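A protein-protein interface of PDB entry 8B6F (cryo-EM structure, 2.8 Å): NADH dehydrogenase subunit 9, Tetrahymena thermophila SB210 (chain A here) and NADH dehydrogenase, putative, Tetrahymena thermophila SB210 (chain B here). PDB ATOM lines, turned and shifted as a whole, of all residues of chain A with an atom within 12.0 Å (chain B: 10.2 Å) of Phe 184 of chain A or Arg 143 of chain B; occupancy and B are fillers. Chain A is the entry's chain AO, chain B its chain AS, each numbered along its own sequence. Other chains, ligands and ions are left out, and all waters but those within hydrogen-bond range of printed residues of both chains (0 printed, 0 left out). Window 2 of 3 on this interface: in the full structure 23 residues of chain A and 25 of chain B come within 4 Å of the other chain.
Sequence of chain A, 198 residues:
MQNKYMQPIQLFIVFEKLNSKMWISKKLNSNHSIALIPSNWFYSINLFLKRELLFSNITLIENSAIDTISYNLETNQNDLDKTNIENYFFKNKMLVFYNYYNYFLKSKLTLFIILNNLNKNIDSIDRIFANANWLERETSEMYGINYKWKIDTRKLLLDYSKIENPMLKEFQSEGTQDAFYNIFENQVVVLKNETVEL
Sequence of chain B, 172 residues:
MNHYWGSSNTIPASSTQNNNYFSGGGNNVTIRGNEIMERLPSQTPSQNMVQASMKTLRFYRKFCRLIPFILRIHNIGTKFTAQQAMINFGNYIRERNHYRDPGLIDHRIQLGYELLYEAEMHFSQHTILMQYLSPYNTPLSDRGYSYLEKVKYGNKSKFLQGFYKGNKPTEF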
ATOM      1  N   PHE A 180     -10.480  20.095  -8.991  1.00  0.00           N
ATOM      2  CA  PHE A 180     -11.857  20.271  -8.554  1.00  0.00           C
ATOM      3  C   PHE A 180     -12.795  19.826  -9.671  1.00  0.00           C
ATOM      4  O   PHE A 180     -12.364  19.320 -10.708  1.00  0.00           O
ATOM      5  CB  PHE A 180     -12.126  21.729  -8.166  1.00  0.00           C
ATOM      6  CG  PHE A 180     -11.343  22.197  -6.977  1.00  0.00           C
ATOM      7  CD1 PHE A 180     -10.070  22.716  -7.131  1.00  0.00           C
ATOM      8  CD2 PHE A 180     -11.888  22.141  -5.706  1.00  0.00           C
ATOM      9  CE1 PHE A 180      -9.350  23.156  -6.037  1.00  0.00           C
ATOM     10  CE2 PHE A 180     -11.173  22.579  -4.609  1.00  0.00           C
ATOM     11  CZ  PHE A 180      -9.903  23.090  -4.778  1.00  0.00           C
ATOM     12  N   TYR A 181     -14.091  20.024  -9.456  1.00  0.00           N
ATOM     13  CA  TYR A 181     -15.105  19.785 -10.472  1.00  0.00           C
ATOM     14  C   TYR A 181     -15.711  21.111 -10.906  1.00  0.00           C
ATOM     15  O   TYR A 181     -16.146  21.902 -10.064  1.00  0.00           O
ATOM     16  CB  TYR A 181     -16.198  18.856  -9.947  1.00  0.00           C
ATOM     17  CG  TYR A 181     -17.385  18.744 -10.870  1.00  0.00           C
ATOM     18  CD1 TYR A 181     -17.353  17.909 -11.976  1.00  0.00           C
ATOM     19  CD2 TYR A 181     -18.540  19.475 -10.635  1.00  0.00           C
ATOM     20  CE1 TYR A 181     -18.438  17.806 -12.823  1.00  0.00           C
ATOM     21  CE2 TYR A 181     -19.630  19.380 -11.473  1.00  0.00           C
ATOM     22  CZ  TYR A 181     -19.574  18.543 -12.566  1.00  0.00           C
ATOM     23  OH  TYR A 181     -20.660  18.447 -13.402  1.00  0.00           O
ATOM     24  N   ASN A 182     -15.742  21.347 -12.216  1.00  0.00           N
ATOM     25  CA  ASN A 182     -16.298  22.569 -12.778  1.00  0.00           C
ATOM     26  C   ASN A 182     -17.678  22.267 -13.352  1.00  0.00           C
ATOM     27  O   ASN A 182     -17.820  21.400 -14.221  1.00  0.00           O
ATOM     28  CB  ASN A 182     -15.370  23.134 -13.850  1.00  0.00           C
ATOM     29  CG  ASN A 182     -15.699  24.566 -14.205  1.00  0.00           C
ATOM     30  OD1 ASN A 182     -16.847  24.995 -14.104  1.00  0.00           O
ATOM     31  ND2 ASN A 182     -14.688  25.318 -14.616  1.00  0.00           N
ATOM     32  N   ILE A 183     -18.688  22.990 -12.866  1.00  0.00           N
ATOM     33  CA  ILE A 183     -20.049  22.841 -13.368  1.00  0.00           C
ATOM     34  C   ILE A 183     -20.169  23.427 -14.765  1.00  0.00           C
ATOM     35  O   ILE A 183     -20.872  22.883 -15.623  1.00  0.00           O
ATOM     36  CB  ILE A 183     -21.044  23.483 -12.382  1.00  0.00           C
ATOM     37  CG1 ILE A 183     -21.101  22.662 -11.090  1.00  0.00           C
ATOM     38  CG2 ILE A 183     -22.434  23.584 -12.993  1.00  0.00           C
ATOM     39  CD1 ILE A 183     -21.742  23.380  -9.926  1.00  0.00           C
ATOM     40  N   PHE A 184     -19.497  24.552 -15.016  1.00  0.00           N
ATOM     41  CA  PHE A 184     -19.567  25.160 -16.339  1.00  0.00           C
ATOM     42  C   PHE A 184     -19.042  24.207 -17.402  1.00  0.00           C
ATOM     43  O   PHE A 184     -19.634  24.076 -18.479  1.00  0.00           O
ATOM     44  CB  PHE A 184     -18.786  26.473 -16.353  1.00  0.00           C
ATOM     45  CG  PHE A 184     -19.322  27.506 -15.403  1.00  0.00           C
ATOM     46  CD1 PHE A 184     -20.489  28.192 -15.690  1.00  0.00           C
ATOM     47  CD2 PHE A 184     -18.651  27.800 -14.228  1.00  0.00           C
ATOM     48  CE1 PHE A 184     -20.983  29.143 -14.821  1.00  0.00           C
ATOM     49  CE2 PHE A 184     -19.139  28.751 -13.352  1.00  0.00           C
ATOM     50  CZ  PHE A 184     -20.305  29.424 -13.651  1.00  0.00           C
ATOM     51  N   GLU A 185     -17.928  23.534 -17.121  1.00  0.00           N
ATOM     52  CA  GLU A 185     -17.406  22.501 -18.003  1.00  0.00           C
ATOM     53  C   GLU A 185     -17.966  21.119 -17.696  1.00  0.00           C
ATOM     54  O   GLU A 185     -17.701  20.179 -18.453  1.00  0.00           O
ATOM     55  CB  GLU A 185     -15.879  22.468 -17.911  1.00  0.00           C
ATOM     56  CG  GLU A 185     -15.233  23.796 -18.271  1.00  0.00           C
ATOM     57  CD  GLU A 185     -13.723  23.760 -18.177  1.00  0.00           C
ATOM     58  OE1 GLU A 185     -13.167  22.662 -17.965  1.00  0.00           O
ATOM     59  OE2 GLU A 185     -13.091  24.827 -18.318  1.00  0.00           O
ATOM     60  N   ASN A 186     -18.728  20.974 -16.613  1.00  0.00           N
ATOM     61  CA  ASN A 186     -19.387  19.713 -16.272  1.00  0.00           C
ATOM     62  C   ASN A 186     -18.390  18.563 -16.203  1.00  0.00           C
ATOM     63  O   ASN A 186     -18.664  17.450 -16.656  1.00  0.00           O
ATOM     64  CB  ASN A 186     -20.502  19.393 -17.267  1.00  0.00           C
ATOM     65  CG  ASN A 186     -21.683  20.330 -17.143  1.00  0.00           C
ATOM     66  OD1 ASN A 186     -22.116  20.659 -16.039  1.00  0.00           O
ATOM     67  ND2 ASN A 186     -22.211  20.769 -18.279  1.00  0.00           N
ATOM     68  N   GLN A 187     -17.220  18.822 -15.628  1.00  0.00           N
ATOM     69  CA  GLN A 187     -16.189  17.794 -15.573  1.00  0.00           C
ATOM     70  C   GLN A 187     -15.093  18.257 -14.623  1.00  0.00           C
ATOM     71  O   GLN A 187     -15.046  19.420 -14.216  1.00  0.00           O
ATOM     72  CB  GLN A 187     -15.636  17.497 -16.970  1.00  0.00           C
ATOM     73  CG  GLN A 187     -14.752  16.261 -17.064  1.00  0.00           C
ATOM     74  CD  GLN A 187     -15.423  15.014 -16.510  1.00  0.00           C
ATOM     75  OE1 GLN A 187     -14.789  14.202 -15.839  1.00  0.00           O
ATOM     76  NE2 GLN A 187     -16.712  14.857 -16.794  1.00  0.00           N
ATOM     77  N   VAL A 188     -14.205  17.323 -14.282  1.00  0.00           N
ATOM     78  CA  VAL A 188     -13.084  17.619 -13.399  1.00  0.00           C
ATOM     79  C   VAL A 188     -12.089  18.515 -14.123  1.00  0.00           C
ATOM     80  O   VAL A 188     -11.714  18.255 -15.273  1.00  0.00           O
ATOM     81  CB  VAL A 188     -12.422  16.319 -12.921  1.00  0.00           C
ATOM     82  CG1 VAL A 188     -11.132  16.606 -12.163  1.00  0.00           C
ATOM     83  CG2 VAL A 188     -13.380  15.533 -12.048  1.00  0.00           C
ATOM     84  N   VAL A 189     -11.661  19.582 -13.448  1.00  0.00           N
ATOM     85  CA  VAL A 189     -10.655  20.500 -13.960  1.00  0.00           C
ATOM     86  C   VAL A 189      -9.562  20.642 -12.908  1.00  0.00           C
ATOM     87  O   VAL A 189      -9.703  20.200 -11.768  1.00  0.00           O
ATOM     88  CB  VAL A 189     -11.247  21.881 -14.319  1.00  0.00           C
ATOM     89  CG1 VAL A 189     -12.476  21.722 -15.188  1.00  0.00           C
ATOM     90  CG2 VAL A 189     -11.586  22.675 -13.060  1.00  0.00           C
ATOM     91  N   VAL A 190      -8.461  21.269 -13.310  1.00  0.00           N
ATOM     92  CA  VAL A 190      -7.329  21.519 -12.427  1.00  0.00           C
ATOM     93  C   VAL A 190      -7.036  23.012 -12.449  1.00  0.00           C
ATOM     94  O   VAL A 190      -6.990  23.624 -13.520  1.00  0.00           O
ATOM     95  CB  VAL A 190      -6.089  20.705 -12.845  1.00  0.00           C
ATOM     96  CG1 VAL A 190      -5.549  21.171 -14.195  1.00  0.00           C
ATOM     97  CG2 VAL A 190      -5.018  20.789 -11.780  1.00  0.00           C
ATOM     98  N   LEU A 191      -6.858  23.599 -11.267  1.00  0.00           N
ATOM     99  CA  LEU A 191      -6.639  25.032 -11.139  1.00  0.00           C
ATOM    100  C   LEU A 191      -5.594  25.279 -10.058  1.00  0.00           C
ATOM    101  O   LEU A 191      -5.087  24.344  -9.430  1.00  0.00           O
ATOM    102  CB  LEU A 191      -7.957  25.760 -10.848  1.00  0.00           C
ATOM    103  CG  LEU A 191      -8.873  25.184  -9.766  1.00  0.00           C
ATOM    104  CD1 LEU A 191      -8.296  25.425  -8.384  1.00  0.00           C
ATOM    105  CD2 LEU A 191     -10.274  25.755  -9.870  1.00  0.00           C
ATOM    106  N   GLY B  77     -13.671  20.629 -30.298  1.00  0.00           N
ATOM    107  CA  GLY B  77     -13.544  21.418 -31.510  1.00  0.00           C
ATOM    108  C   GLY B  77     -14.196  22.781 -31.399  1.00  0.00           C
ATOM    109  O   GLY B  77     -13.707  23.756 -31.974  1.00  0.00           O
ATOM    110  N   THR B  78     -15.310  22.868 -30.669  1.00  0.00           N
ATOM    111  CA  THR B  78     -15.998  24.146 -30.517  1.00  0.00           C
ATOM    112  C   THR B  78     -15.140  25.151 -29.759  1.00  0.00           C
ATOM    113  O   THR B  78     -15.136  26.344 -30.083  1.00  0.00           O
ATOM    114  CB  THR B  78     -17.330  23.937 -29.797  1.00  0.00           C
ATOM    115  OG1 THR B  78     -18.080  22.913 -30.463  1.00  0.00           O
ATOM    116  CG2 THR B  78     -18.144  25.222 -29.785  1.00  0.00           C
ATOM    117  N   LYS B  79     -14.409  24.690 -28.742  1.00  0.00           N
ATOM    118  CA  LYS B  79     -13.616  25.605 -27.928  1.00  0.00           C
ATOM    119  C   LYS B  79     -12.569  26.326 -28.765  1.00  0.00           C
ATOM    120  O   LYS B  79     -12.319  27.520 -28.564  1.00  0.00           O
ATOM    121  CB  LYS B  79     -12.951  24.842 -26.782  1.00  0.00           C
ATOM    122  CG  LYS B  79     -13.924  24.357 -25.719  1.00  0.00           C
ATOM    123  CD  LYS B  79     -13.225  23.505 -24.673  1.00  0.00           C
ATOM    124  CE  LYS B  79     -14.187  23.076 -23.577  1.00  0.00           C
ATOM    125  NZ  LYS B  79     -15.321  22.266 -24.108  1.00  0.00           N
ATOM    126  N   PHE B  80     -11.941  25.621 -29.699  1.00  0.00           N
ATOM    127  CA  PHE B  80     -10.930  26.226 -30.555  1.00  0.00           C
ATOM    128  C   PHE B  80     -10.838  25.434 -31.849  1.00  0.00           C
ATOM    129  O   PHE B  80     -11.077  24.226 -31.871  1.00  0.00           O
ATOM    130  CB  PHE B  80      -9.567  26.276 -29.857  1.00  0.00           C
ATOM    131  CG  PHE B  80      -9.377  25.201 -28.826  1.00  0.00           C
ATOM    132  CD1 PHE B  80      -9.296  23.872 -29.200  1.00  0.00           C
ATOM    133  CD2 PHE B  80      -9.266  25.523 -27.485  1.00  0.00           C
ATOM    134  CE1 PHE B  80      -9.121  22.883 -28.253  1.00  0.00           C
ATOM    135  CE2 PHE B  80      -9.090  24.539 -26.534  1.00  0.00           C
ATOM    136  CZ  PHE B  80      -9.018  23.217 -26.919  1.00  0.00           C
ATOM    137  N   HIS B 126     -10.493  15.768 -21.314  1.00  0.00           N
ATOM    138  CA  HIS B 126     -10.439  16.907 -22.225  1.00  0.00           C
ATOM    139  C   HIS B 126     -10.223  18.209 -21.462  1.00  0.00           C
ATOM    140  O   HIS B 126      -9.435  19.060 -21.887  1.00  0.00           O
ATOM    141  CB  HIS B 126     -11.706  16.967 -23.082  1.00  0.00           C
ATOM    142  CG  HIS B 126     -12.951  17.299 -22.320  1.00  0.00           C
ATOM    143  ND1 HIS B 126     -13.598  16.385 -21.516  1.00  0.00           N
ATOM    144  CD2 HIS B 126     -13.688  18.433 -22.269  1.00  0.00           C
ATOM    145  CE1 HIS B 126     -14.670  16.950 -20.987  1.00  0.00           C
ATOM    146  NE2 HIS B 126     -14.749  18.191 -21.431  1.00  0.00           N
ATOM    147  N   THR B 127     -10.919  18.388 -20.337  1.00  0.00           N
ATOM    148  CA  THR B 127     -10.756  19.612 -19.560  1.00  0.00           C
ATOM    149  C   THR B 127      -9.367  19.714 -18.946  1.00  0.00           C
ATOM    150  O   THR B 127      -8.864  20.824 -18.736  1.00  0.00           O
ATOM    151  CB  THR B 127     -11.813  19.692 -18.458  1.00  0.00           C
ATOM    152  OG1 THR B 127     -11.690  18.562 -17.586  1.00  0.00           O
ATOM    153  CG2 THR B 127     -13.203  19.717 -19.050  1.00  0.00           C
ATOM    154  N   MET B 130      -6.822  20.361 -22.199  1.00  0.00           N
ATOM    155  CA  MET B 130      -7.006  21.549 -23.020  1.00  0.00           C
ATOM    156  C   MET B 130      -6.241  22.751 -22.488  1.00  0.00           C
ATOM    157  O   MET B 130      -6.216  23.789 -23.159  1.00  0.00           O
ATOM    158  CB  MET B 130      -8.492  21.896 -23.126  1.00  0.00           C
ATOM    159  CG  MET B 130      -9.125  22.351 -21.821  1.00  0.00           C
ATOM    160  SD  MET B 130     -10.872  22.741 -22.022  1.00  0.00           S
ATOM    161  CE  MET B 130     -11.254  23.407 -20.407  1.00  0.00           C
ATOM    162  N   SER B 134      -5.285  25.914 -24.886  1.00  0.00           N
ATOM    163  CA  SER B 134      -6.090  27.101 -24.654  1.00  0.00           C
ATOM    164  C   SER B 134      -5.353  28.357 -25.118  1.00  0.00           C
ATOM    165  O   SER B 134      -4.125  28.435 -25.029  1.00  0.00           O
ATOM    166  CB  SER B 134      -6.434  27.230 -23.174  1.00  0.00           C
ATOM    167  OG  SER B 134      -7.144  26.094 -22.714  1.00  0.00           O
ATOM    168  N   PRO B 135      -6.079  29.363 -25.611  1.00  0.00           N
ATOM    169  CA  PRO B 135      -5.419  30.609 -26.014  1.00  0.00           C
ATOM    170  C   PRO B 135      -4.786  31.317 -24.825  1.00  0.00           C
ATOM    171  O   PRO B 135      -5.277  31.247 -23.697  1.00  0.00           O
ATOM    172  CB  PRO B 135      -6.558  31.443 -26.615  1.00  0.00           C
ATOM    173  CG  PRO B 135      -7.636  30.473 -26.922  1.00  0.00           C
ATOM    174  CD  PRO B 135      -7.524  29.398 -25.897  1.00  0.00           C
ATOM    175  N   THR B 138      -6.721  35.150 -25.737  1.00  0.00           N
ATOM    176  CA  THR B 138      -7.957  35.232 -26.493  1.00  0.00           C
ATOM    177  C   THR B 138      -9.061  34.442 -25.794  1.00  0.00           C
ATOM    178  O   THR B 138      -8.787  33.416 -25.164  1.00  0.00           O
ATOM    179  CB  THR B 138      -7.760  34.682 -27.913  1.00  0.00           C
ATOM    180  OG1 THR B 138      -6.665  35.358 -28.544  1.00  0.00           O
ATOM    181  CG2 THR B 138      -9.017  34.866 -28.752  1.00  0.00           C
ATOM    182  N   PRO B 139     -10.312  34.890 -25.873  1.00  0.00           N
ATOM    183  CA  PRO B 139     -11.397  34.129 -25.245  1.00  0.00           C
ATOM    184  C   PRO B 139     -11.599  32.773 -25.900  1.00  0.00           C
ATOM    185  O   PRO B 139     -11.322  32.576 -27.085  1.00  0.00           O
ATOM    186  CB  PRO B 139     -12.624  35.024 -25.447  1.00  0.00           C
ATOM    187  CG  PRO B 139     -12.084  36.377 -25.679  1.00  0.00           C
ATOM    188  CD  PRO B 139     -10.791  36.180 -26.397  1.00  0.00           C
ATOM    189  N   LEU B 140     -12.089  31.830 -25.102  1.00  0.00           N
ATOM    190  CA  LEU B 140     -12.473  30.530 -25.631  1.00  0.00           C
ATOM    191  C   LEU B 140     -13.677  30.687 -26.555  1.00  0.00           C
ATOM    192  O   LEU B 140     -14.594  31.462 -26.276  1.00  0.00           O
ATOM    193  CB  LEU B 140     -12.795  29.569 -24.487  1.00  0.00           C
ATOM    194  CG  LEU B 140     -12.370  28.107 -24.655  1.00  0.00           C
ATOM    195  CD1 LEU B 140     -10.860  27.981 -24.818  1.00  0.00           C
ATOM    196  CD2 LEU B 140     -12.841  27.278 -23.473  1.00  0.00           C
ATOM    197  N   SER B 141     -13.670  29.944 -27.663  1.00  0.00           N
ATOM    198  CA  SER B 141     -14.652  30.160 -28.719  1.00  0.00           C
ATOM    199  C   SER B 141     -16.040  29.635 -28.376  1.00  0.00           C
ATOM    200  O   SER B 141     -16.991  29.946 -29.101  1.00  0.00           O
ATOM    201  CB  SER B 141     -14.176  29.503 -30.017  1.00  0.00           C
ATOM    202  OG  SER B 141     -12.928  30.030 -30.431  1.00  0.00           O
ATOM    203  N   ASP B 142     -16.189  28.856 -27.309  1.00  0.00           N
ATOM    204  CA  ASP B 142     -17.475  28.277 -26.940  1.00  0.00           C
ATOM    205  C   ASP B 142     -18.161  29.038 -25.814  1.00  0.00           C
ATOM    206  O   ASP B 142     -19.173  28.563 -25.290  1.00  0.00           O
ATOM    207  CB  ASP B 142     -17.296  26.813 -26.540  1.00  0.00           C
ATOM    208  CG  ASP B 142     -16.441  26.651 -25.305  1.00  0.00           C
ATOM    209  OD1 ASP B 142     -15.499  27.452 -25.130  1.00  0.00           O
ATOM    210  OD2 ASP B 142     -16.706  25.725 -24.510  1.00  0.00           O
ATOM    211  N   ARG B 143     -17.640  30.199 -25.432  1.00  0.00           N
ATOM    212  CA  ARG B 143     -18.166  30.962 -24.312  1.00  0.00           C
ATOM    213  C   ARG B 143     -18.275  32.429 -24.694  1.00  0.00           C
ATOM    214  O   ARG B 143     -17.569  32.918 -25.579  1.00  0.00           O
ATOM    215  CB  ARG B 143     -17.273  30.829 -23.070  1.00  0.00           C
ATOM    216  CG  ARG B 143     -17.153  29.421 -22.525  1.00  0.00           C
ATOM    217  CD  ARG B 143     -15.992  29.323 -21.549  1.00  0.00           C
ATOM    218  NE  ARG B 143     -15.996  28.066 -20.812  1.00  0.00           N
ATOM    219  CZ  ARG B 143     -16.630  27.868 -19.666  1.00  0.00           C
ATOM    220  NH1 ARG B 143     -17.338  28.828 -19.090  1.00  0.00           N
ATOM    221  NH2 ARG B 143     -16.554  26.677 -19.079  1.00  0.00           N
ATOM    222  N   GLY B 144     -19.178  33.127 -24.016  1.00  0.00           N
ATOM    223  CA  GLY B 144     -19.265  34.565 -24.147  1.00  0.00           C
ATOM    224  C   GLY B 144     -18.334  35.250 -23.172  1.00  0.00           C
ATOM    225  O   GLY B 144     -18.402  35.003 -21.965  1.00  0.00           O
ATOM    226  N   TYR B 145     -17.456  36.108 -23.678  1.00  0.00           N
ATOM    227  CA  TYR B 145     -16.451  36.744 -22.843  1.00  0.00           C
ATOM    228  C   TYR B 145     -16.965  38.061 -22.277  1.00  0.00           C
ATOM    229  O   TYR B 145     -17.923  38.655 -22.775  1.00  0.00           O
ATOM    230  CB  TYR B 145     -15.164  36.979 -23.633  1.00  0.00           C
ATOM    231  CG  TYR B 145     -15.337  37.828 -24.869  1.00  0.00           C
ATOM    232  CD1 TYR B 145     -15.252  39.210 -24.806  1.00  0.00           C
ATOM    233  CD2 TYR B 145     -15.569  37.242 -26.104  1.00  0.00           C
ATOM    234  CE1 TYR B 145     -15.404  39.985 -25.936  1.00  0.00           C
ATOM    235  CE2 TYR B 145     -15.722  38.007 -27.238  1.00  0.00           C
ATOM    236  CZ  TYR B 145     -15.638  39.378 -27.149  1.00  0.00           C
ATOM    237  OH  TYR B 145     -15.790  40.144 -28.280  1.00  0.00           O
ATOM    238  N   SER B 146     -16.303  38.512 -21.218  1.00  0.00           N
ATOM    239  CA  SER B 146     -16.628  39.761 -20.544  1.00  0.00           C
ATOM    240  C   SER B 146     -15.506  40.756 -20.796  1.00  0.00           C
ATOM    241  O   SER B 146     -14.350  40.492 -20.446  1.00  0.00           O
ATOM    242  CB  SER B 146     -16.818  39.533 -19.045  1.00  0.00           C
ATOM    243  OG  SER B 146     -16.907  40.762 -18.346  1.00  0.00           O
ATOM    244  N   TYR B 147     -15.847  41.895 -21.397  1.00  0.00           N
ATOM    245  CA  TYR B 147     -14.898  42.975 -21.637  1.00  0.00           C
ATOM    246  C   TYR B 147     -15.114  44.139 -20.675  1.00  0.00           C
ATOM    247  O   TYR B 147     -14.720  45.269 -20.974  1.00  0.00           O
ATOM    248  CB  TYR B 147     -14.985  43.453 -23.087  1.00  0.00           C
ATOM    249  CG  TYR B 147     -16.383  43.787 -23.550  1.00  0.00           C
ATOM    250  CD1 TYR B 147     -17.198  42.819 -24.118  1.00  0.00           C
ATOM    251  CD2 TYR B 147     -16.884  45.073 -23.428  1.00  0.00           C
ATOM    252  CE1 TYR B 147     -18.476  43.122 -24.544  1.00  0.00           C
ATOM    253  CE2 TYR B 147     -18.159  45.388 -23.850  1.00  0.00           C
ATOM    254  CZ  TYR B 147     -18.950  44.408 -24.408  1.00  0.00           C
ATOM    255  OH  TYR B 147     -20.220  44.717 -24.829  1.00  0.00           O
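The side-chain carboxylate (OE2) of Glu 185 of chain A is in salt-bridge range of the guanidinium group (NH2) of Arg 143 of chain B, at 3.999 Å.
The backbone carbonyl oxygen (O) of Val 188 of chain A lies close to the side-chain hydroxyl (OG1) of Thr 127 of chain B (2.3 Å).
Arg 143 of chain B touches Phe 184 of chain A (NH2 to CB, 3.5 Å).
CG2 of Thr 127 of chain B touches OE1 of Glu 185 of chain A, at 3.1 Å.
Met 130 of chain B touches Glu 185 of chain A (CE to OE2, 3.1 Å).
CG of Gln 187 of chain A touches CE1 of His 126 of chain B, 3.98 Å away.
Thr 127 of chain B touches Gln 187 of chain A (OG1 to CG, 3.9 Å).
Thr 127 of chain B touches Val 189 of chain A.
Hydrophobic or aromatic side chains of chain A that line the printed part of chain B: Phe 184 and Val 189.
Hydrophobic or aromatic side chains of chain B that line the printed part of chain A: His 126 and Met 130.
Among the printed residues, 8 pairs touch across the chains.
Of chain B, only Arg 143 (3.5 Å) comes within 4 Å of Phe 184 of chain A.
Arg 143 of chain B touches just these residues of chain A: Phe 184 and Glu 185.
No residue of chain B comes within 4 Å of Asn 182 of chain A.
Of chain B, only Thr 127, Met 130 and Arg 143 come within 4 Å of Glu 185 of chain A.
No residue of chain A comes within 4 Å of Pro 139 of chain B.
No residue of chain A comes within 4 Å of Leu 140 of chain B.
Ser 141 of chain B touches none of the printed residues of chain A.
No residue of chain A comes within 4 Å of Asp 142 of chain B.
No residue of chain A comes within 4 Å of Gly 144 of chain B.
No residue of chain A comes within 4 Å of Tyr 145 of chain B.
Of the printed residues of chain A, Thr 127 of chain B touches Glu 185, Gln 187, Val 188 and Val 189.
Of the printed residues of chain A, His 126 of chain B touches Gln 187 (3.98 Å).
Of the printed residues of chain A, Met 130 of chain B touches Glu 185 (3.1 Å).
Printed residues of chain B within 4 Å of Val 188 of chain A: Thr 127 (2.3 Å).
The nearest residue of chain B that does not touch Phe 184 of chain A is Asp 142 of chain B (6.9 Å).
The nearest residue of chain A that does not touch Arg 143 of chain B is Asn 182 of chain A (5.0 Å).
The nearest printed residue of chain B that does not touch Gln 187 of chain A is Met 130 of chain B (8.1 Å).
The backbone NH (N) of Val 189 of chain A sits at hydrogen-bond distance from the backbone carbonyl oxygen (O) of Phe 180 of chain A (2.8 Å).
OD1 of Asn 182 of chain A lies within hydrogen-bond range of N of Phe 184 of chain A, 2.8 Å away.
The backbone carbonyl oxygen (O) of Gln 187 of chain A sits at hydrogen-bond distance from the backbone NH (N) of Asn 182 of chain A, at 2.9 Å.
The backbone carbonyl oxygen (O) of Met 130 of chain B sits at hydrogen-bond distance from the side-chain hydroxyl (OG) of Ser 134 of chain B (2.5 Å).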
